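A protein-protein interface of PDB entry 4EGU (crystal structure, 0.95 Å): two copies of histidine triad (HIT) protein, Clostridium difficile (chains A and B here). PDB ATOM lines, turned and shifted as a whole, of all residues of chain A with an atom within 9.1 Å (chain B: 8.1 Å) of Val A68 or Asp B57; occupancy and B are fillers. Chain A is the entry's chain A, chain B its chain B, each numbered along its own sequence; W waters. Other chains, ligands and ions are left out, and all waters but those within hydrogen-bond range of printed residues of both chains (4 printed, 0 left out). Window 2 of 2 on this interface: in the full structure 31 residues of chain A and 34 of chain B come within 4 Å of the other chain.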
ATOM      1  N   TYR A  22     -39.078 -28.279  19.178  1.00  0.00           N
ATOM      2  CA  TYR A  22     -38.710 -27.276  18.193  1.00  0.00           C
ATOM      3  C   TYR A  22     -38.989 -27.822  16.813  1.00  0.00           C
ATOM      4  O   TYR A  22     -38.757 -29.012  16.560  1.00  0.00           O
ATOM      5  CB  TYR A  22     -37.216 -26.951  18.300  1.00  0.00           C
ATOM      6  CG  TYR A  22     -36.737 -25.941  17.283  1.00  0.00           C
ATOM      7  CD1 TYR A  22     -36.715 -24.587  17.592  1.00  0.00           C
ATOM      8  CD2 TYR A  22     -36.342 -26.323  16.014  1.00  0.00           C
ATOM      9  CE1 TYR A  22     -36.289 -23.656  16.674  1.00  0.00           C
ATOM     10  CE2 TYR A  22     -35.925 -25.385  15.073  1.00  0.00           C
ATOM     11  CZ  TYR A  22     -35.910 -24.039  15.420  1.00  0.00           C
ATOM     12  OH  TYR A  22     -35.488 -23.063  14.544  1.00  0.00           O
ATOM     13  N   ASP A  24     -38.454 -26.229  12.586  1.00  0.00           N
ATOM     14  CA  ASP A  24     -38.427 -25.287  11.480  1.00  0.00           C
ATOM     15  C   ASP A  24     -38.314 -26.098  10.185  1.00  0.00           C
ATOM     16  O   ASP A  24     -38.580 -27.315  10.180  1.00  0.00           O
ATOM     17  CB  ASP A  24     -37.347 -24.195  11.666  1.00  0.00           C
ATOM     18  CG  ASP A  24     -35.909 -24.717  11.615  1.00  0.00           C
ATOM     19  OD1 ASP A  24     -35.667 -25.827  11.129  1.00  0.00           O
ATOM     20  OD2 ASP A  24     -35.012 -23.952  12.071  1.00  0.00           O
ATOM     21  N   ARG A  26     -35.793 -27.121   8.603  1.00  0.00           N
ATOM     22  CA  ARG A  26     -34.517 -27.860   8.524  1.00  0.00           C
ATOM     23  C   ARG A  26     -34.274 -28.822   9.675  1.00  0.00           C
ATOM     24  O   ARG A  26     -33.498 -29.753   9.515  1.00  0.00           O
ATOM     25  CB  ARG A  26     -33.313 -26.899   8.558  1.00  0.00           C
ATOM     26  CG  ARG A  26     -33.048 -26.131   7.283  1.00  0.00           C
ATOM     27  CD  ARG A  26     -31.830 -25.218   7.436  1.00  0.00           C
ATOM     28  NE  ARG A  26     -30.570 -25.949   7.326  1.00  0.00           N
ATOM     29  CZ  ARG A  26     -29.379 -25.447   7.644  1.00  0.00           C
ATOM     30  NH1 ARG A  26     -29.275 -24.208   8.104  1.00  0.00           N
ATOM     31  NH2 ARG A  26     -28.288 -26.186   7.502  1.00  0.00           N
ATOM     32  N   VAL A  27     -34.808 -28.512  10.857  1.00  0.00           N
ATOM     33  CA  VAL A  27     -34.446 -29.170  12.107  1.00  0.00           C
ATOM     34  C   VAL A  27     -35.705 -29.421  12.905  1.00  0.00           C
ATOM     35  O   VAL A  27     -36.644 -28.624  12.901  1.00  0.00           O
ATOM     36  CB  VAL A  27     -33.449 -28.281  12.913  1.00  0.00           C
ATOM     37  CG1 VAL A  27     -33.328 -28.740  14.357  1.00  0.00           C
ATOM     38  CG2 VAL A  27     -32.066 -28.274  12.248  1.00  0.00           C
ATOM     39  N   VAL A  43     -31.968 -33.187  19.083  1.00  0.00           N
ATOM     40  CA  VAL A  43     -32.045 -32.199  18.026  1.00  0.00           C
ATOM     41  C   VAL A  43     -31.509 -32.837  16.759  1.00  0.00           C
ATOM     42  O   VAL A  43     -30.373 -33.323  16.752  1.00  0.00           O
ATOM     43  CB  VAL A  43     -31.242 -30.916  18.359  1.00  0.00           C
ATOM     44  CG1 VAL A  43     -31.516 -29.857  17.318  1.00  0.00           C
ATOM     45  CG2 VAL A  43     -31.606 -30.393  19.747  1.00  0.00           C
ATOM     46  N   ASP A  61     -22.520 -26.443   8.190  1.00  0.00           N
ATOM     47  CA  ASP A  61     -23.398 -25.428   8.724  1.00  0.00           C
ATOM     48  C   ASP A  61     -24.657 -26.014   9.366  1.00  0.00           C
ATOM     49  O   ASP A  61     -25.270 -25.350  10.196  1.00  0.00           O
ATOM     50  CB  ASP A  61     -23.760 -24.364   7.674  1.00  0.00           C
ATOM     51  CG  ASP A  61     -24.329 -24.944   6.376  1.00  0.00           C
ATOM     52  OD1 ASP A  61     -24.516 -26.173   6.240  1.00  0.00           O
ATOM     53  OD2 ASP A  61     -24.593 -24.133   5.464  1.00  0.00           O
ATOM     54  N   ILE A  62     -25.047 -27.249   9.031  1.00  0.00           N
ATOM     55  CA  ILE A  62     -26.185 -27.834   9.733  1.00  0.00           C
ATOM     56  C   ILE A  62     -25.883 -27.931  11.226  1.00  0.00           C
ATOM     57  O   ILE A  62     -26.786 -27.798  12.061  1.00  0.00           O
ATOM     58  CB  ILE A  62     -26.603 -29.188   9.119  1.00  0.00           C
ATOM     59  CG1 ILE A  62     -27.917 -29.683   9.731  1.00  0.00           C
ATOM     60  CG2 ILE A  62     -25.529 -30.237   9.276  1.00  0.00           C
ATOM     61  CD1 ILE A  62     -29.107 -28.750   9.571  1.00  0.00           C
ATOM     62  N   VAL A  63     -24.620 -28.164  11.583  1.00  0.00           N
ATOM     63  CA  VAL A  63     -24.239 -28.243  12.996  1.00  0.00           C
ATOM     64  C   VAL A  63     -24.352 -26.862  13.671  1.00  0.00           C
ATOM     65  O   VAL A  63     -24.791 -26.773  14.823  1.00  0.00           O
ATOM     66  CB  VAL A  63     -22.844 -28.877  13.159  1.00  0.00           C
ATOM     67  CG1 VAL A  63     -22.405 -28.865  14.614  1.00  0.00           C
ATOM     68  CG2 VAL A  63     -22.862 -30.305  12.623  1.00  0.00           C
ATOM     69  N   SER A  64     -23.983 -25.785  12.990  1.00  0.00           N
ATOM     70  CA  SER A  64     -24.164 -24.463  13.562  1.00  0.00           C
ATOM     71  C   SER A  64     -25.662 -24.166  13.758  1.00  0.00           C
ATOM     72  O   SER A  64     -26.045 -23.636  14.800  1.00  0.00           O
ATOM     73  CB  SER A  64     -23.445 -23.391  12.775  1.00  0.00           C
ATOM     74  OG  SER A  64     -23.892 -23.342  11.485  1.00  0.00           O
ATOM     75  N   HIS A  65     -26.490 -24.539  12.781  1.00  0.00           N
ATOM     76  CA  HIS A  65     -27.906 -24.296  12.944  1.00  0.00           C
ATOM     77  C   HIS A  65     -28.471 -25.102  14.126  1.00  0.00           C
ATOM     78  O   HIS A  65     -29.265 -24.561  14.909  1.00  0.00           O
ATOM     79  CB  HIS A  65     -28.682 -24.569  11.668  1.00  0.00           C
ATOM     80  CG  HIS A  65     -30.101 -24.120  11.775  1.00  0.00           C
ATOM     81  ND1 HIS A  65     -30.469 -22.820  12.066  1.00  0.00           N
ATOM     82  CD2 HIS A  65     -31.249 -24.824  11.699  1.00  0.00           C
ATOM     83  CE1 HIS A  65     -31.788 -22.742  12.116  1.00  0.00           C
ATOM     84  NE2 HIS A  65     -32.286 -23.946  11.885  1.00  0.00           N
ATOM     85  N   ILE A  66     -28.050 -26.352  14.264  1.00  0.00           N
ATOM     86  CA  ILE A  66     -28.447 -27.138  15.411  1.00  0.00           C
ATOM     87  C   ILE A  66     -28.084 -26.438  16.718  1.00  0.00           C
ATOM     88  O   ILE A  66     -28.859 -26.467  17.669  1.00  0.00           O
ATOM     89  CB  ILE A  66     -27.845 -28.546  15.302  1.00  0.00           C
ATOM     90  CG1 ILE A  66     -28.621 -29.361  14.249  1.00  0.00           C
ATOM     91  CG2 ILE A  66     -27.782 -29.255  16.645  1.00  0.00           C
ATOM     92  CD1 ILE A  66     -27.956 -30.693  13.883  1.00  0.00           C
ATOM     93  N   HIS A  67     -26.897 -25.831  16.780  1.00  0.00           N
ATOM     94  CA  HIS A  67     -26.475 -25.135  17.996  1.00  0.00           C
ATOM     95  C   HIS A  67     -27.257 -23.843  18.267  1.00  0.00           C
ATOM     96  O   HIS A  67     -27.515 -23.532  19.426  1.00  0.00           O
ATOM     97  CB  HIS A  67     -24.975 -24.913  18.003  1.00  0.00           C
ATOM     98  CG  HIS A  67     -24.211 -26.153  18.385  1.00  0.00           C
ATOM     99  ND1 HIS A  67     -24.047 -27.244  17.567  1.00  0.00           N
ATOM    100  CD2 HIS A  67     -23.614 -26.493  19.555  1.00  0.00           C
ATOM    101  CE1 HIS A  67     -23.365 -28.181  18.225  1.00  0.00           C
ATOM    102  NE2 HIS A  67     -23.086 -27.748  19.435  1.00  0.00           N
ATOM    103  N   VAL A  68     -27.646 -23.099  17.228  1.00  0.00           N
ATOM    104  CA  VAL A  68     -28.567 -21.986  17.434  1.00  0.00           C
ATOM    105  C   VAL A  68     -29.878 -22.509  18.051  1.00  0.00           C
ATOM    106  O   VAL A  68     -30.410 -21.908  18.986  1.00  0.00           O
ATOM    107  CB  VAL A  68     -28.822 -21.222  16.120  1.00  0.00           C
ATOM    108  CG1 VAL A  68     -29.982 -20.236  16.297  1.00  0.00           C
ATOM    109  CG2 VAL A  68     -27.549 -20.514  15.688  1.00  0.00           C
ATOM    110  N   VAL A  69     -30.386 -23.624  17.526  1.00  0.00           N
ATOM    111  CA  VAL A  69     -31.605 -24.231  18.054  1.00  0.00           C
ATOM    112  C   VAL A  69     -31.434 -24.633  19.525  1.00  0.00           C
ATOM    113  O   VAL A  69     -32.320 -24.364  20.335  1.00  0.00           O
ATOM    114  CB  VAL A  69     -32.045 -25.399  17.162  1.00  0.00           C
ATOM    115  CG1 VAL A  69     -33.162 -26.209  17.815  1.00  0.00           C
ATOM    116  CG2 VAL A  69     -32.456 -24.873  15.788  1.00  0.00           C
ATOM    117  N   ILE A  70     -30.309 -25.265  19.854  1.00  0.00           N
ATOM    118  CA  ILE A  70     -30.054 -25.642  21.240  1.00  0.00           C
ATOM    119  C   ILE A  70     -30.142 -24.409  22.143  1.00  0.00           C
ATOM    120  O   ILE A  70     -30.800 -24.443  23.184  1.00  0.00           O
ATOM    121  CB  ILE A  70     -28.676 -26.331  21.355  1.00  0.00           C
ATOM    122  CG1 ILE A  70     -28.715 -27.706  20.688  1.00  0.00           C
ATOM    123  CG2 ILE A  70     -28.229 -26.413  22.816  1.00  0.00           C
ATOM    124  CD1 ILE A  70     -27.357 -28.361  20.512  1.00  0.00           C
ATOM    125  N   ASN A  71     -29.461 -23.336  21.763  1.00  0.00           N
ATOM    126  CA  ASN A  71     -29.456 -22.140  22.591  1.00  0.00           C
ATOM    127  C   ASN A  71     -30.862 -21.511  22.674  1.00  0.00           C
ATOM    128  O   ASN A  71     -31.242 -21.000  23.731  1.00  0.00           O
ATOM    129  CB  ASN A  71     -28.448 -21.114  22.107  1.00  0.00           C
ATOM    130  CG  ASN A  71     -27.050 -21.394  22.596  1.00  0.00           C
ATOM    131  OD1 ASN A  71     -26.779 -22.386  23.287  1.00  0.00           O
ATOM    132  ND2 ASN A  71     -26.146 -20.491  22.259  1.00  0.00           N
ATOM    133  N   LYS A  72     -31.629 -21.558  21.585  1.00  0.00           N
ATOM    134  CA  LYS A  72     -32.992 -21.024  21.613  1.00  0.00           C
ATOM    135  C   LYS A  72     -33.856 -21.798  22.597  1.00  0.00           C
ATOM    136  O   LYS A  72     -34.669 -21.199  23.314  1.00  0.00           O
ATOM    137  CB  LYS A  72     -33.611 -21.071  20.213  1.00  0.00           C
ATOM    138  CG  LYS A  72     -33.106 -19.971  19.296  1.00  0.00           C
ATOM    139  CD  LYS A  72     -33.728 -20.025  17.917  1.00  0.00           C
ATOM    140  CE  LYS A  72     -33.539 -18.728  17.148  1.00  0.00           C
ATOM    141  NZ  LYS A  72     -34.196 -17.596  17.818  1.00  0.00           N
ATOM    142  N   ILE A  73     -33.724 -23.122  22.611  1.00  0.00           N
ATOM    143  CA  ILE A  73     -34.479 -23.949  23.532  1.00  0.00           C
ATOM    144  C   ILE A  73     -34.043 -23.648  24.965  1.00  0.00           C
ATOM    145  O   ILE A  73     -34.881 -23.472  25.855  1.00  0.00           O
ATOM    146  CB  ILE A  73     -34.320 -25.442  23.182  1.00  0.00           C
ATOM    147  CG1 ILE A  73     -34.915 -25.777  21.815  1.00  0.00           C
ATOM    148  CG2 ILE A  73     -34.937 -26.327  24.260  1.00  0.00           C
ATOM    149  CD1 ILE A  73     -34.467 -27.132  21.283  1.00  0.00           C
ATOM    150  N   ALA A  74     -32.736 -23.560  25.189  1.00  0.00           N
ATOM    151  CA  ALA A  74     -32.223 -23.258  26.521  1.00  0.00           C
ATOM    152  C   ALA A  74     -32.799 -21.950  27.050  1.00  0.00           C
ATOM    153  O   ALA A  74     -33.172 -21.854  28.216  1.00  0.00           O
ATOM    154  CB  ALA A  74     -30.711 -23.198  26.497  1.00  0.00           C
ATOM    155  N   LYS A  75     -32.814 -20.928  26.205  1.00  0.00           N
ATOM    156  CA  LYS A  75     -33.305 -19.608  26.632  1.00  0.00           C
ATOM    157  C   LYS A  75     -34.787 -19.626  26.942  1.00  0.00           C
ATOM    158  O   LYS A  75     -35.225 -19.031  27.906  1.00  0.00           O
ATOM    159  CB  LYS A  75     -32.958 -18.550  25.588  1.00  0.00           C
ATOM    160  CG  LYS A  75     -31.462 -18.260  25.487  1.00  0.00           C
ATOM    161  CD  LYS A  75     -31.036 -17.391  24.294  1.00  0.00           C
ATOM    162  CE  LYS A  75     -29.499 -17.301  24.126  1.00  0.00           C
ATOM    163  NZ  LYS A  75     -29.043 -16.580  22.886  1.00  0.00           N
ATOM    164  N   GLU A  76     -35.578 -20.315  26.138  1.00  0.00           N
ATOM    165  CA  GLU A  76     -37.003 -20.434  26.372  1.00  0.00           C
ATOM    166  C   GLU A  76     -37.296 -21.148  27.679  1.00  0.00           C
ATOM    167  O   GLU A  76     -38.146 -20.756  28.460  1.00  0.00           O
ATOM    168  CB  GLU A  76     -37.606 -21.270  25.281  1.00  0.00           C
ATOM    169  CG  GLU A  76     -39.072 -21.482  25.460  1.00  0.00           C
ATOM    170  CD  GLU A  76     -39.589 -22.547  24.527  1.00  0.00           C
ATOM    171  OE1 GLU A  76     -38.788 -23.408  24.113  1.00  0.00           O
ATOM    172  OE2 GLU A  76     -40.782 -22.527  24.184  1.00  0.00           O
ATOM    173  N   PHE A  84     -26.240 -26.786  30.925  1.00  0.00           N
ATOM    174  CA  PHE A  84     -26.685 -27.921  30.133  1.00  0.00           C
ATOM    175  C   PHE A  84     -25.470 -28.579  29.488  1.00  0.00           C
ATOM    176  O   PHE A  84     -24.390 -28.004  29.472  1.00  0.00           O
ATOM    177  CB  PHE A  84     -27.732 -27.503  29.075  1.00  0.00           C
ATOM    178  CG  PHE A  84     -27.285 -26.442  28.108  1.00  0.00           C
ATOM    179  CD1 PHE A  84     -27.399 -25.095  28.410  1.00  0.00           C
ATOM    180  CD2 PHE A  84     -26.795 -26.798  26.860  1.00  0.00           C
ATOM    181  CE1 PHE A  84     -27.037 -24.126  27.501  1.00  0.00           C
ATOM    182  CE2 PHE A  84     -26.427 -25.831  25.940  1.00  0.00           C
ATOM    183  CZ  PHE A  84     -26.548 -24.492  26.259  1.00  0.00           C
ATOM    184  N   ILE A 105     -29.370 -32.883  24.224  1.00  0.00           N
ATOM    185  CA  ILE A 105     -29.274 -31.830  25.224  1.00  0.00           C
ATOM    186  C   ILE A 105     -29.731 -32.431  26.548  1.00  0.00           C
ATOM    187  O   ILE A 105     -30.841 -32.955  26.634  1.00  0.00           O
ATOM    188  CB  ILE A 105     -30.195 -30.626  24.944  1.00  0.00           C
ATOM    189  CG1 ILE A 105     -30.162 -30.115  23.506  1.00  0.00           C
ATOM    190  CG2 ILE A 105     -29.857 -29.495  25.917  1.00  0.00           C
ATOM    191  CD1 ILE A 105     -31.273 -29.077  23.239  1.00  0.00           C
ATOM    192  N   LEU B  52     -20.977 -21.930  25.500  1.00  0.00           N
ATOM    193  CA  LEU B  52     -21.826 -22.029  24.333  1.00  0.00           C
ATOM    194  C   LEU B  52     -22.970 -21.017  24.378  1.00  0.00           C
ATOM    195  O   LEU B  52     -23.306 -20.402  23.377  1.00  0.00           O
ATOM    196  CB  LEU B  52     -22.369 -23.465  24.253  1.00  0.00           C
ATOM    197  CG  LEU B  52     -23.383 -23.801  23.178  1.00  0.00           C
ATOM    198  CD1 LEU B  52     -22.888 -23.439  21.793  1.00  0.00           C
ATOM    199  CD2 LEU B  52     -23.727 -25.272  23.249  1.00  0.00           C
ATOM    200  N   ILE B  53     -23.589 -20.856  25.542  1.00  0.00           N
ATOM    201  CA  ILE B  53     -24.770 -20.031  25.648  1.00  0.00           C
ATOM    202  C   ILE B  53     -24.424 -18.565  25.489  1.00  0.00           C
ATOM    203  O   ILE B  53     -25.321 -17.757  25.256  1.00  0.00           O
ATOM    204  CB  ILE B  53     -25.546 -20.334  26.986  1.00  0.00           C
ATOM    205  CG1 ILE B  53     -26.990 -19.822  26.963  1.00  0.00           C
ATOM    206  CG2 ILE B  53     -24.784 -19.757  28.181  1.00  0.00           C
ATOM    207  CD1 ILE B  53     -27.835 -20.375  25.858  1.00  0.00           C
ATOM    208  N   ASP B  54     -23.141 -18.217  25.603  1.00  0.00           N
ATOM    209  CA  ASP B  54     -22.662 -16.856  25.408  1.00  0.00           C
ATOM    210  C   ASP B  54     -22.231 -16.543  23.961  1.00  0.00           C
ATOM    211  O   ASP B  54     -21.874 -15.400  23.682  1.00  0.00           O
ATOM    212  CB  ASP B  54     -21.508 -16.600  26.374  1.00  0.00           C
ATOM    213  CG  ASP B  54     -21.952 -16.683  27.832  1.00  0.00           C
ATOM    214  OD1 ASP B  54     -22.906 -15.984  28.224  1.00  0.00           O
ATOM    215  OD2 ASP B  54     -21.363 -17.478  28.582  1.00  0.00           O
ATOM    216  N   ILE B  55     -22.281 -17.511  23.040  1.00  0.00           N
ATOM    217  CA  ILE B  55     -21.979 -17.239  21.631  1.00  0.00           C
ATOM    218  C   ILE B  55     -23.245 -16.647  20.991  1.00  0.00           C
ATOM    219  O   ILE B  55     -24.278 -17.310  20.975  1.00  0.00           O
ATOM    220  CB  ILE B  55     -21.599 -18.521  20.864  1.00  0.00           C
ATOM    221  CG1 ILE B  55     -20.439 -19.300  21.500  1.00  0.00           C
ATOM    222  CG2 ILE B  55     -21.231 -18.171  19.417  1.00  0.00           C
ATOM    223  CD1 ILE B  55     -20.238 -20.684  20.827  1.00  0.00           C
ATOM    224  N   PRO B  56     -23.184 -15.429  20.443  1.00  0.00           N
ATOM    225  CA  PRO B  56     -24.371 -14.923  19.754  1.00  0.00           C
ATOM    226  C   PRO B  56     -24.747 -15.825  18.577  1.00  0.00           C
ATOM    227  O   PRO B  56     -23.865 -16.402  17.918  1.00  0.00           O
ATOM    228  CB  PRO B  56     -23.930 -13.532  19.278  1.00  0.00           C
ATOM    229  CG  PRO B  56     -22.837 -13.142  20.232  1.00  0.00           C
ATOM    230  CD  PRO B  56     -22.109 -14.436  20.494  1.00  0.00           C
ATOM    231  N   ASP B  57     -26.038 -15.905  18.265  1.00  0.00           N
ATOM    232  CA  ASP B  57     -26.478 -16.683  17.124  1.00  0.00           C
ATOM    233  C   ASP B  57     -25.676 -16.326  15.880  1.00  0.00           C
ATOM    234  O   ASP B  57     -25.312 -17.218  15.134  1.00  0.00           O
ATOM    235  CB  ASP B  57     -27.980 -16.439  16.812  1.00  0.00           C
ATOM    236  CG  ASP B  57     -28.932 -16.914  17.888  1.00  0.00           C
ATOM    237  OD1 ASP B  57     -28.536 -17.686  18.780  1.00  0.00           O
ATOM    238  OD2 ASP B  57     -30.102 -16.506  17.795  1.00  0.00           O
ATOM    239  N   LYS B  58     -25.414 -15.036  15.659  1.00  0.00           N
ATOM    240  CA  LYS B  58     -24.731 -14.593  14.448  1.00  0.00           C
ATOM    241  C   LYS B  58     -23.290 -15.089  14.334  1.00  0.00           C
ATOM    242  O   LYS B  58     -22.701 -15.024  13.247  1.00  0.00           O
ATOM    243  CB  LYS B  58     -24.753 -13.058  14.350  1.00  0.00           C
ATOM    244  CG  LYS B  58     -26.135 -12.500  13.997  1.00  0.00           C
ATOM    245  CD  LYS B  58     -26.212 -10.979  14.136  1.00  0.00           C
ATOM    246  CE  LYS B  58     -27.653 -10.486  13.964  1.00  0.00           C
ATOM    247  NZ  LYS B  58     -27.781  -9.027  14.226  1.00  0.00           N
ATOM    248  N   GLU B  59     -22.721 -15.594  15.435  1.00  0.00           N
ATOM    249  CA  GLU B  59     -21.332 -16.058  15.507  1.00  0.00           C
ATOM    250  C   GLU B  59     -21.228 -17.569  15.656  1.00  0.00           C
ATOM    251  O   GLU B  59     -20.119 -18.107  15.799  1.00  0.00           O
ATOM    252  CB  GLU B  59     -20.619 -15.345  16.653  1.00  0.00           C
ATOM    253  CG  GLU B  59     -20.505 -13.821  16.403  1.00  0.00           C
ATOM    254  CD  GLU B  59     -19.988 -13.053  17.586  1.00  0.00           C
ATOM    255  OE1 GLU B  59     -19.049 -13.540  18.211  1.00  0.00           O
ATOM    256  OE2 GLU B  59     -20.531 -11.971  17.910  1.00  0.00           O
ATOM    257  N   MET B  60     -22.362 -18.272  15.611  1.00  0.00           N
ATOM    258  CA  MET B  60     -22.379 -19.696  15.950  1.00  0.00           C
ATOM    259  C   MET B  60     -21.586 -20.572  14.977  1.00  0.00           C
ATOM    260  O   MET B  60     -21.271 -21.710  15.310  1.00  0.00           O
ATOM    261  CB  MET B  60     -23.816 -20.210  16.050  1.00  0.00           C
ATOM    262  CG  MET B  60     -23.934 -21.534  16.778  1.00  0.00           C
ATOM    263  SD  MET B  60     -23.350 -21.526  18.459  1.00  0.00           S
ATOM    264  CE  MET B  60     -24.653 -20.536  19.219  1.00  0.00           C
ATOM    265  N   ASP B  61     -21.207 -20.078  13.783  1.00  0.00           N
ATOM    266  CA  ASP B  61     -20.413 -20.912  12.881  1.00  0.00           C
ATOM    267  C   ASP B  61     -19.007 -21.305  13.392  1.00  0.00           C
ATOM    268  O   ASP B  61     -18.376 -22.225  12.846  1.00  0.00           O
ATOM    269  CB  ASP B  61     -20.433 -20.345  11.466  1.00  0.00           C
ATOM    270  CG  ASP B  61     -21.818 -20.421  10.839  1.00  0.00           C
ATOM    271  OD1 ASP B  61     -22.198 -21.497  10.299  1.00  0.00           O
ATOM    272  OD2 ASP B  61     -22.559 -19.434  10.925  1.00  0.00           O
ATOM    273  N   ILE B  62     -18.519 -20.694  14.468  1.00  0.00           N
ATOM    274  CA  ILE B  62     -17.330 -21.238  15.124  1.00  0.00           C
ATOM    275  C   ILE B  62     -17.531 -22.709  15.501  1.00  0.00           C
ATOM    276  O   ILE B  62     -16.591 -23.506  15.440  1.00  0.00           O
ATOM    277  CB  ILE B  62     -16.892 -20.376  16.327  1.00  0.00           C
ATOM    278  CG1 ILE B  62     -15.556 -20.847  16.905  1.00  0.00           C
ATOM    279  CG2 ILE B  62     -17.949 -20.332  17.401  1.00  0.00           C
ATOM    280  CD1 ILE B  62     -14.390 -20.937  15.920  1.00  0.00           C
ATOM    281  N   VAL B  63     -18.757 -23.084  15.859  1.00  0.00           N
ATOM    282  CA  VAL B  63     -19.036 -24.475  16.245  1.00  0.00           C
ATOM    283  C   VAL B  63     -18.965 -25.393  15.020  1.00  0.00           C
ATOM    284  O   VAL B  63     -18.456 -26.513  15.109  1.00  0.00           O
ATOM    285  CB  VAL B  63     -20.370 -24.594  16.973  1.00  0.00           C
ATOM    286  CG1 VAL B  63     -20.702 -26.032  17.286  1.00  0.00           C
ATOM    287  CG2 VAL B  63     -20.343 -23.789  18.251  1.00  0.00           C
HETATM  288  O   HOH W   1     -30.244 -18.112  20.963  1.00  0.00           O
HETATM  289  O   HOH W   2     -26.180 -16.441  23.163  1.00  0.00           O
HETATM  290  O   HOH W   3     -32.122 -16.728  19.445  1.00  0.00           O
HETATM  291  O   HOH W   4     -26.844 -18.035  20.852  1.00  0.00           O
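Asp B57 touches one residue of chain A. Printed residues of chain A within 4 Å of Asp B61: Ser A64. Printed residues of chain A within 4 Å of Met B60: Ser A64, His A67, Val A68 and Asn A71. Val A69 touches none of the printed residues of chain B. The nearest residue of chain A that does not touch Asp B57 is Lys A72 (4.1 Å).
O of Leu B52 is in hydrogen-bond range of ND2 of Asn A71. The side-chain hydroxyl (OG) of Ser A64 lies within hydrogen-bond range of the side-chain carboxylate (OD1) of Asp B61, at 2.8 Å.
Positions printed for both chains: 61, 62 and 63.
Water W3 lies within hydrogen-bond range of OD2 of Asp B57 and NZ of Lys A72. Water W2 lies within hydrogen-bond range of O of Ile B53 (2.6 Å), NZ of Lys A75 (2.9 Å) and O of Ile B55 (3.0 Å). Water W4 lies within hydrogen-bond range of the backbone carbonyl oxygen of Ile B55 (2.7 Å), the side-chain carboxylate of Asp B57 (2.7 Å), the side-chain amide nitrogen of Asn A71 (2.9 Å) and the side-chain amino group of Lys A75 (3.3 Å). Water W1 bridges NZ of Lys A75 (2.7 Å) and OD1 of Asp B57 (2.8 Å).
O of Val A63 lies within hydrogen-bond range of ND1 of His A67, at 2.9 Å. O of Asp A61 is in hydrogen-bond range of OG of Ser A64 (2.8 Å).
Of the 23 printed residues of chain A, 6 touch a printed residue of chain B. Hydrophobic or aromatic side chains of chain B within 4 Å of the printed part of chain A: Leu B52, Ile B53, Met B60 and Val B63. Among the printed residues, 13 pairs touch across the chains.
Ser A64 touches Met B60 (O to CG, 3.6 Å). Leu B52 touches His A67. Met B60 touches His A67. Val B63 touches His A67. CG2 of Val A68 touches CB of Met B60 (3.8 Å). Asn A71 touches Ile B53. O of Ile B55 touches ND2 of Asn A71 (3.9 Å). Asn A71 touches Met B60 (ND2 to CE, 3.4 Å). Ile B53 touches Lys A75. CD2 of Leu B52 touches CE2 of Phe A84, at 3.9 Å.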
